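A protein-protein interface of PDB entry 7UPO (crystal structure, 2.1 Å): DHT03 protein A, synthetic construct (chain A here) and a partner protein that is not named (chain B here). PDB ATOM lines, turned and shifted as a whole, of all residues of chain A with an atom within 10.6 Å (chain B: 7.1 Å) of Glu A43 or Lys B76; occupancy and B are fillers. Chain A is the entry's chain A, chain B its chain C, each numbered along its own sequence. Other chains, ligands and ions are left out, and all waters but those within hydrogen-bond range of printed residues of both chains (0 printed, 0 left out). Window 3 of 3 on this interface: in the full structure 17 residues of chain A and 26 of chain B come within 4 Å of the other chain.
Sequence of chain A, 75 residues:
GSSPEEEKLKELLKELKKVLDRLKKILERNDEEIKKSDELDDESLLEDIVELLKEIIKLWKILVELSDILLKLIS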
ATOM      1  N   ARG A  29      13.970 -35.617   6.969  1.00  0.00           N
ATOM      2  CA  ARG A  29      13.354 -35.720   5.648  1.00  0.00           C
ATOM      3  C   ARG A  29      13.851 -34.613   4.727  1.00  0.00           C
ATOM      4  O   ARG A  29      14.195 -34.863   3.566  1.00  0.00           O
ATOM      5  CB  ARG A  29      11.830 -35.671   5.762  1.00  0.00           C
ATOM      6  CG  ARG A  29      11.122 -36.001   4.458  1.00  0.00           C
ATOM      7  CD  ARG A  29       9.681 -35.517   4.437  1.00  0.00           C
ATOM      8  NE  ARG A  29       9.582 -34.079   4.189  1.00  0.00           N
ATOM      9  CZ  ARG A  29       9.137 -33.193   5.075  1.00  0.00           C
ATOM     10  NH1 ARG A  29       8.737 -33.593   6.274  1.00  0.00           N
ATOM     11  NH2 ARG A  29       9.083 -31.907   4.758  1.00  0.00           N
ATOM     12  N   ASN A  30      13.889 -33.377   5.230  1.00  0.00           N
ATOM     13  CA  ASN A  30      14.398 -32.264   4.435  1.00  0.00           C
ATOM     14  C   ASN A  30      15.857 -32.484   4.060  1.00  0.00           C
ATOM     15  O   ASN A  30      16.253 -32.270   2.909  1.00  0.00           O
ATOM     16  CB  ASN A  30      14.231 -30.953   5.202  1.00  0.00           C
ATOM     17  CG  ASN A  30      12.782 -30.534   5.320  1.00  0.00           C
ATOM     18  OD1 ASN A  30      11.878 -31.249   4.884  1.00  0.00           O
ATOM     19  ND2 ASN A  30      12.551 -29.370   5.916  1.00  0.00           N
ATOM     20  N   GLU A  33      15.879 -35.178   1.401  1.00  0.00           N
ATOM     21  CA  GLU A  33      15.420 -34.732   0.089  1.00  0.00           C
ATOM     22  C   GLU A  33      16.440 -33.828  -0.592  1.00  0.00           C
ATOM     23  O   GLU A  33      16.583 -33.872  -1.818  1.00  0.00           O
ATOM     24  CB  GLU A  33      14.078 -34.011   0.220  1.00  0.00           C
ATOM     25  CG  GLU A  33      12.914 -34.908   0.619  1.00  0.00           C
ATOM     26  CD  GLU A  33      12.283 -35.611  -0.569  1.00  0.00           C
ATOM     27  OE1 GLU A  33      12.171 -34.981  -1.642  1.00  0.00           O
ATOM     28  OE2 GLU A  33      11.901 -36.792  -0.433  1.00  0.00           O
ATOM     29  N   GLU A  39      19.820 -30.415  -9.524  1.00  0.00           N
ATOM     30  CA  GLU A  39      18.838 -29.342  -9.485  1.00  0.00           C
ATOM     31  C   GLU A  39      17.779 -29.611  -8.424  1.00  0.00           C
ATOM     32  O   GLU A  39      17.363 -30.753  -8.213  1.00  0.00           O
ATOM     33  CB  GLU A  39      18.184 -29.181 -10.856  1.00  0.00           C
ATOM     34  CG  GLU A  39      17.766 -30.493 -11.498  1.00  0.00           C
ATOM     35  CD  GLU A  39      17.516 -30.358 -12.986  1.00  0.00           C
ATOM     36  OE1 GLU A  39      17.698 -29.245 -13.524  1.00  0.00           O
ATOM     37  OE2 GLU A  39      17.143 -31.367 -13.620  1.00  0.00           O
ATOM     38  N   LEU A  40      17.347 -28.547  -7.756  1.00  0.00           N
ATOM     39  CA  LEU A  40      16.337 -28.620  -6.708  1.00  0.00           C
ATOM     40  C   LEU A  40      15.065 -27.936  -7.183  1.00  0.00           C
ATOM     41  O   LEU A  40      15.118 -26.836  -7.743  1.00  0.00           O
ATOM     42  CB  LEU A  40      16.830 -27.968  -5.412  1.00  0.00           C
ATOM     43  CG  LEU A  40      17.949 -28.653  -4.622  1.00  0.00           C
ATOM     44  CD1 LEU A  40      19.315 -28.373  -5.228  1.00  0.00           C
ATOM     45  CD2 LEU A  40      17.915 -28.228  -3.161  1.00  0.00           C
ATOM     46  N   ASP A  41      13.927 -28.587  -6.961  1.00  0.00           N
ATOM     47  CA  ASP A  41      12.648 -27.998  -7.327  1.00  0.00           C
ATOM     48  C   ASP A  41      12.284 -26.880  -6.359  1.00  0.00           C
ATOM     49  O   ASP A  41      12.495 -26.988  -5.147  1.00  0.00           O
ATOM     50  CB  ASP A  41      11.550 -29.062  -7.340  1.00  0.00           C
ATOM     51  CG  ASP A  41      10.229 -28.531  -7.860  1.00  0.00           C
ATOM     52  OD1 ASP A  41      10.216 -27.432  -8.454  1.00  0.00           O
ATOM     53  OD2 ASP A  41       9.197 -29.210  -7.672  1.00  0.00           O
ATOM     54  N   ASP A  42      11.728 -25.799  -6.906  1.00  0.00           N
ATOM     55  CA  ASP A  42      11.391 -24.641  -6.089  1.00  0.00           C
ATOM     56  C   ASP A  42      10.138 -24.882  -5.257  1.00  0.00           C
ATOM     57  O   ASP A  42      10.065 -24.448  -4.102  1.00  0.00           O
ATOM     58  CB  ASP A  42      11.205 -23.417  -6.983  1.00  0.00           C
ATOM     59  CG  ASP A  42      12.383 -23.186  -7.905  1.00  0.00           C
ATOM     60  OD1 ASP A  42      13.496 -23.643  -7.572  1.00  0.00           O
ATOM     61  OD2 ASP A  42      12.196 -22.552  -8.965  1.00  0.00           O
ATOM     62  N   GLU A  43       9.144 -25.565  -5.828  1.00  0.00           N
ATOM     63  CA  GLU A  43       7.895 -25.803  -5.111  1.00  0.00           C
ATOM     64  C   GLU A  43       8.121 -26.691  -3.894  1.00  0.00           C
ATOM     65  O   GLU A  43       7.712 -26.351  -2.778  1.00  0.00           O
ATOM     66  CB  GLU A  43       6.864 -26.429  -6.051  1.00  0.00           C
ATOM     67  CG  GLU A  43       5.522 -26.711  -5.395  1.00  0.00           C
ATOM     68  CD  GLU A  43       4.597 -27.519  -6.284  1.00  0.00           C
ATOM     69  OE1 GLU A  43       5.098 -28.193  -7.210  1.00  0.00           O
ATOM     70  OE2 GLU A  43       3.370 -27.480  -6.059  1.00  0.00           O
ATOM     71  N   SER A  44       8.776 -27.839  -4.091  1.00  0.00           N
ATOM     72  CA  SER A  44       9.016 -28.755  -2.982  1.00  0.00           C
ATOM     73  C   SER A  44       9.938 -28.143  -1.935  1.00  0.00           C
ATOM     74  O   SER A  44       9.821 -28.462  -0.747  1.00  0.00           O
ATOM     75  CB  SER A  44       9.601 -30.067  -3.501  1.00  0.00           C
ATOM     76  OG  SER A  44      10.813 -29.841  -4.201  1.00  0.00           O
ATOM     77  N   LEU A  45      10.854 -27.267  -2.351  1.00  0.00           N
ATOM     78  CA  LEU A  45      11.750 -26.621  -1.397  1.00  0.00           C
ATOM     79  C   LEU A  45      10.972 -25.706  -0.459  1.00  0.00           C
ATOM     80  O   LEU A  45      11.176 -25.727   0.760  1.00  0.00           O
ATOM     81  CB  LEU A  45      12.830 -25.839  -2.143  1.00  0.00           C
ATOM     82  CG  LEU A  45      14.217 -25.817  -1.505  1.00  0.00           C
ATOM     83  CD1 LEU A  45      14.730 -27.235  -1.321  1.00  0.00           C
ATOM     84  CD2 LEU A  45      15.181 -25.006  -2.357  1.00  0.00           C
ATOM     85  N   LEU A  46      10.067 -24.897  -1.013  1.00  0.00           N
ATOM     86  CA  LEU A  46       9.248 -24.022  -0.182  1.00  0.00           C
ATOM     87  C   LEU A  46       8.238 -24.812   0.641  1.00  0.00           C
ATOM     88  O   LEU A  46       7.919 -24.418   1.768  1.00  0.00           O
ATOM     89  CB  LEU A  46       8.536 -22.987  -1.053  1.00  0.00           C
ATOM     90  CG  LEU A  46       9.442 -22.002  -1.792  1.00  0.00           C
ATOM     91  CD1 LEU A  46       8.626 -21.056  -2.657  1.00  0.00           C
ATOM     92  CD2 LEU A  46      10.300 -21.226  -0.804  1.00  0.00           C
ATOM     93  N   GLU A  47       7.731 -25.926   0.105  1.00  0.00           N
ATOM     94  CA  GLU A  47       6.801 -26.753   0.868  1.00  0.00           C
ATOM     95  C   GLU A  47       7.490 -27.404   2.061  1.00  0.00           C
ATOM     96  O   GLU A  47       6.910 -27.483   3.150  1.00  0.00           O
ATOM     97  CB  GLU A  47       6.176 -27.816  -0.035  1.00  0.00           C
ATOM     98  CG  GLU A  47       5.185 -27.272  -1.049  1.00  0.00           C
ATOM     99  CD  GLU A  47       4.725 -28.333  -2.030  1.00  0.00           C
ATOM    100  OE1 GLU A  47       5.288 -29.448  -2.009  1.00  0.00           O
ATOM    101  OE2 GLU A  47       3.800 -28.056  -2.820  1.00  0.00           O
ATOM    102  N   ASP A  48       8.726 -27.881   1.875  1.00  0.00           N
ATOM    103  CA  ASP A  48       9.487 -28.413   3.001  1.00  0.00           C
ATOM    104  C   ASP A  48       9.768 -27.328   4.032  1.00  0.00           C
ATOM    105  O   ASP A  48       9.764 -27.591   5.240  1.00  0.00           O
ATOM    106  CB  ASP A  48      10.795 -29.037   2.510  1.00  0.00           C
ATOM    107  CG  ASP A  48      10.572 -30.267   1.648  1.00  0.00           C
ATOM    108  OD1 ASP A  48       9.402 -30.576   1.345  1.00  0.00           O
ATOM    109  OD2 ASP A  48      11.567 -30.926   1.277  1.00  0.00           O
ATOM    110  N   ILE A  49      10.013 -26.099   3.571  1.00  0.00           N
ATOM    111  CA  ILE A  49      10.199 -24.979   4.490  1.00  0.00           C
ATOM    112  C   ILE A  49       8.908 -24.687   5.242  1.00  0.00           C
ATOM    113  O   ILE A  49       8.923 -24.416   6.449  1.00  0.00           O
ATOM    114  CB  ILE A  49      10.700 -23.740   3.723  1.00  0.00           C
ATOM    115  CG1 ILE A  49      12.149 -23.940   3.271  1.00  0.00           C
ATOM    116  CG2 ILE A  49      10.563 -22.487   4.574  1.00  0.00           C
ATOM    117  CD1 ILE A  49      12.678 -22.810   2.419  1.00  0.00           C
ATOM    118  N   VAL A  50       7.771 -24.740   4.541  1.00  0.00           N
ATOM    119  CA  VAL A  50       6.481 -24.482   5.180  1.00  0.00           C
ATOM    120  C   VAL A  50       6.245 -25.467   6.317  1.00  0.00           C
ATOM    121  O   VAL A  50       5.838 -25.083   7.421  1.00  0.00           O
ATOM    122  CB  VAL A  50       5.345 -24.536   4.140  1.00  0.00           C
ATOM    123  CG1 VAL A  50       4.005 -24.745   4.822  1.00  0.00           C
ATOM    124  CG2 VAL A  50       5.319 -23.259   3.311  1.00  0.00           C
ATOM    125  N   GLU A  51       6.510 -26.753   6.071  1.00  0.00           N
ATOM    126  CA  GLU A  51       6.293 -27.760   7.104  1.00  0.00           C
ATOM    127  C   GLU A  51       7.251 -27.571   8.274  1.00  0.00           C
ATOM    128  O   GLU A  51       6.883 -27.816   9.429  1.00  0.00           O
ATOM    129  CB  GLU A  51       6.436 -29.161   6.510  1.00  0.00           C
ATOM    130  CG  GLU A  51       6.057 -30.274   7.475  1.00  0.00           C
ATOM    131  CD  GLU A  51       6.069 -31.643   6.827  1.00  0.00           C
ATOM    132  OE1 GLU A  51       6.187 -31.716   5.585  1.00  0.00           O
ATOM    133  OE2 GLU A  51       5.957 -32.648   7.561  1.00  0.00           O
ATOM    134  N   LYS A  54       6.030 -24.518  10.413  1.00  0.00           N
ATOM    135  CA  LYS A  54       4.834 -24.808  11.200  1.00  0.00           C
ATOM    136  C   LYS A  54       5.187 -25.487  12.520  1.00  0.00           C
ATOM    137  O   LYS A  54       4.695 -25.094  13.584  1.00  0.00           O
ATOM    138  CB  LYS A  54       3.871 -25.675  10.391  1.00  0.00           C
ATOM    139  CG  LYS A  54       3.189 -24.932   9.253  1.00  0.00           C
ATOM    140  CD  LYS A  54       2.243 -25.837   8.477  1.00  0.00           C
ATOM    141  CE  LYS A  54       1.452 -25.036   7.462  1.00  0.00           C
ATOM    142  NZ  LYS A  54       0.762 -23.881   8.103  1.00  0.00           N
ATOM    143  N   LYS B   3      13.096 -18.535  -7.763  1.00  0.00           N
ATOM    144  CA  LYS B   3      12.486 -19.000  -6.520  1.00  0.00           C
ATOM    145  C   LYS B   3      13.494 -19.700  -5.618  1.00  0.00           C
ATOM    146  O   LYS B   3      13.295 -19.760  -4.400  1.00  0.00           O
ATOM    147  CB  LYS B   3      11.316 -19.928  -6.830  1.00  0.00           C
ATOM    148  CG  LYS B   3      10.219 -19.272  -7.643  1.00  0.00           C
ATOM    149  CD  LYS B   3       9.428 -20.310  -8.428  1.00  0.00           C
ATOM    150  CE  LYS B   3       8.414 -19.659  -9.361  1.00  0.00           C
ATOM    151  NZ  LYS B   3       7.825 -20.626 -10.336  1.00  0.00           N
ATOM    152  N   ILE B  71       4.167 -16.954  -1.758  1.00  0.00           N
ATOM    153  CA  ILE B  71       4.910 -17.425  -2.923  1.00  0.00           C
ATOM    154  C   ILE B  71       4.362 -18.767  -3.395  1.00  0.00           C
ATOM    155  O   ILE B  71       4.126 -18.970  -4.591  1.00  0.00           O
ATOM    156  CB  ILE B  71       6.411 -17.514  -2.600  1.00  0.00           C
ATOM    157  CG1 ILE B  71       6.905 -16.195  -2.007  1.00  0.00           C
ATOM    158  CG2 ILE B  71       7.200 -17.854  -3.851  1.00  0.00           C
ATOM    159  CD1 ILE B  71       8.164 -16.337  -1.191  1.00  0.00           C
ATOM    160  N   LEU B  72       4.156 -19.700  -2.461  1.00  0.00           N
ATOM    161  CA  LEU B  72       3.630 -21.013  -2.824  1.00  0.00           C
ATOM    162  C   LEU B  72       2.269 -20.902  -3.497  1.00  0.00           C
ATOM    163  O   LEU B  72       1.988 -21.617  -4.464  1.00  0.00           O
ATOM    164  CB  LEU B  72       3.534 -21.904  -1.586  1.00  0.00           C
ATOM    165  CG  LEU B  72       4.700 -22.854  -1.320  1.00  0.00           C
ATOM    166  CD1 LEU B  72       4.375 -23.767  -0.151  1.00  0.00           C
ATOM    167  CD2 LEU B  72       5.020 -23.665  -2.564  1.00  0.00           C
ATOM    168  N   TYR B  73       1.407 -20.015  -2.994  1.00  0.00           N
ATOM    169  CA  TYR B  73       0.095 -19.841  -3.607  1.00  0.00           C
ATOM    170  C   TYR B  73       0.221 -19.319  -5.031  1.00  0.00           C
ATOM    171  O   TYR B  73      -0.515 -19.749  -5.926  1.00  0.00           O
ATOM    172  CB  TYR B  73      -0.762 -18.894  -2.765  1.00  0.00           C
ATOM    173  CG  TYR B  73      -2.182 -18.766  -3.261  1.00  0.00           C
ATOM    174  CD1 TYR B  73      -2.530 -17.797  -4.194  1.00  0.00           C
ATOM    175  CD2 TYR B  73      -3.176 -19.619  -2.801  1.00  0.00           C
ATOM    176  CE1 TYR B  73      -3.826 -17.681  -4.653  1.00  0.00           C
ATOM    177  CE2 TYR B  73      -4.477 -19.509  -3.256  1.00  0.00           C
ATOM    178  CZ  TYR B  73      -4.793 -18.538  -4.181  1.00  0.00           C
ATOM    179  OH  TYR B  73      -6.084 -18.424  -4.636  1.00  0.00           O
ATOM    180  N   LYS B  74       1.150 -18.389  -5.262  1.00  0.00           N
ATOM    181  CA  LYS B  74       1.344 -17.872  -6.611  1.00  0.00           C
ATOM    182  C   LYS B  74       2.033 -18.892  -7.509  1.00  0.00           C
ATOM    183  O   LYS B  74       1.786 -18.913  -8.720  1.00  0.00           O
ATOM    184  CB  LYS B  74       2.139 -16.567  -6.567  1.00  0.00           C
ATOM    185  CG  LYS B  74       1.398 -15.414  -5.907  1.00  0.00           C
ATOM    186  CD  LYS B  74       2.195 -14.121  -5.998  1.00  0.00           C
ATOM    187  CE  LYS B  74       1.429 -12.956  -5.390  1.00  0.00           C
ATOM    188  NZ  LYS B  74       2.165 -11.671  -5.538  1.00  0.00           N
ATOM    189  N   VAL B  75       2.890 -19.744  -6.941  1.00  0.00           N
ATOM    190  CA  VAL B  75       3.550 -20.774  -7.739  1.00  0.00           C
ATOM    191  C   VAL B  75       2.540 -21.817  -8.202  1.00  0.00           C
ATOM    192  O   VAL B  75       2.480 -22.165  -9.389  1.00  0.00           O
ATOM    193  CB  VAL B  75       4.702 -21.418  -6.945  1.00  0.00           C
ATOM    194  CG1 VAL B  75       5.172 -22.693  -7.630  1.00  0.00           C
ATOM    195  CG2 VAL B  75       5.858 -20.442  -6.801  1.00  0.00           C
ATOM    196  N   LYS B  76       1.727 -22.328  -7.277  1.00  0.00           N
ATOM    197  CA  LYS B  76       0.723 -23.333  -7.605  1.00  0.00           C
ATOM    198  C   LYS B  76      -0.428 -22.782  -8.433  1.00  0.00           C
ATOM    199  O   LYS B  76      -1.294 -23.561  -8.844  1.00  0.00           O
ATOM    200  CB  LYS B  76       0.165 -23.957  -6.325  1.00  0.00           C
ATOM    201  CG  LYS B  76       1.183 -24.685  -5.467  1.00  0.00           C
ATOM    202  CD  LYS B  76       0.516 -25.227  -4.214  1.00  0.00           C
ATOM    203  CE  LYS B  76       1.499 -25.970  -3.335  1.00  0.00           C
ATOM    204  NZ  LYS B  76       0.839 -26.529  -2.122  1.00  0.00           N
ATOM    205  N   SER B  77      -0.465 -21.477  -8.684  1.00  0.00           N
ATOM    206  CA  SER B  77      -1.580 -20.853  -9.389  1.00  0.00           C
ATOM    207  C   SER B  77      -1.529 -21.109 -10.893  1.00  0.00           C
ATOM    208  O   SER B  77      -1.972 -20.279 -11.687  1.00  0.00           O
ATOM    209  CB  SER B  77      -1.599 -19.348  -9.118  1.00  0.00           C
ATOM    210  OG  SER B  77      -2.677 -18.722  -9.792  1.00  0.00           O
ATOM    211  OXT SER B  77      -1.047 -22.143 -11.355  1.00  0.00           O
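The side-chain amino group (NZ) of Lys B76 lies within salt-bridge range of the side-chain carboxylate (OE2) of Glu A47 (3.4 Å).
The backbone NH of Glu A43 is in hydrogen-bond range of the side-chain carboxylate of Asp A41 (3.4 Å).
CB of Asp A42 touches CB of Lys B3 (3.5 Å).
CD2 of Leu B72 touches O of Glu A43 (3.8 Å).
Glu A43 touches Lys B76.
Leu A46 touches Ile B71 (CD1 to CG2, 3.7 Å).
CG of Leu B72 touches CB of Leu A46 (3.8 Å).
CD1 of Leu B72 touches CG of Glu A47, at 3.7 Å.
Val A50 touches Leu B72.
Printed residues of chain B within 4 Å of Glu A43: Leu B72 and Lys B76.
Leu A45 touches none of the printed residues of chain B.
Printed residues of chain B within 4 Å of Glu A47: Leu B72 (3.7 Å) and Lys B76 (3.1 Å).
Of the printed residues of chain B, Val A50 touches Leu B72.
Printed residues of chain A within 4 Å of Lys B3: Asp A42.
Printed residues of chain A within 4 Å of Ile B71: Leu A46 (3.7 Å).
Of the printed residues of chain A, Lys B76 touches Glu A43 and Glu A47.
No residue of chain A comes within 4 Å of Ser B77.
The nearest residue of chain B that does not touch Glu A43 is Val B75 (4.4 Å).
The nearest residue of chain A that does not touch Lys B76 is Ser A44 (7.6 Å).
Of the 17 printed residues of chain A, 5 touch a printed residue of chain B.
Hydrophobic or aromatic side chains of chain B within 4 Å of the printed part of chain A: Ile B71 and Leu B72.
Among the printed residues, Asp or Glu carboxylates within 4 Å of a Lys or Arg side-chain nitrogen of the other chain: Glu A47 with Lys B76 (3.4 Å).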
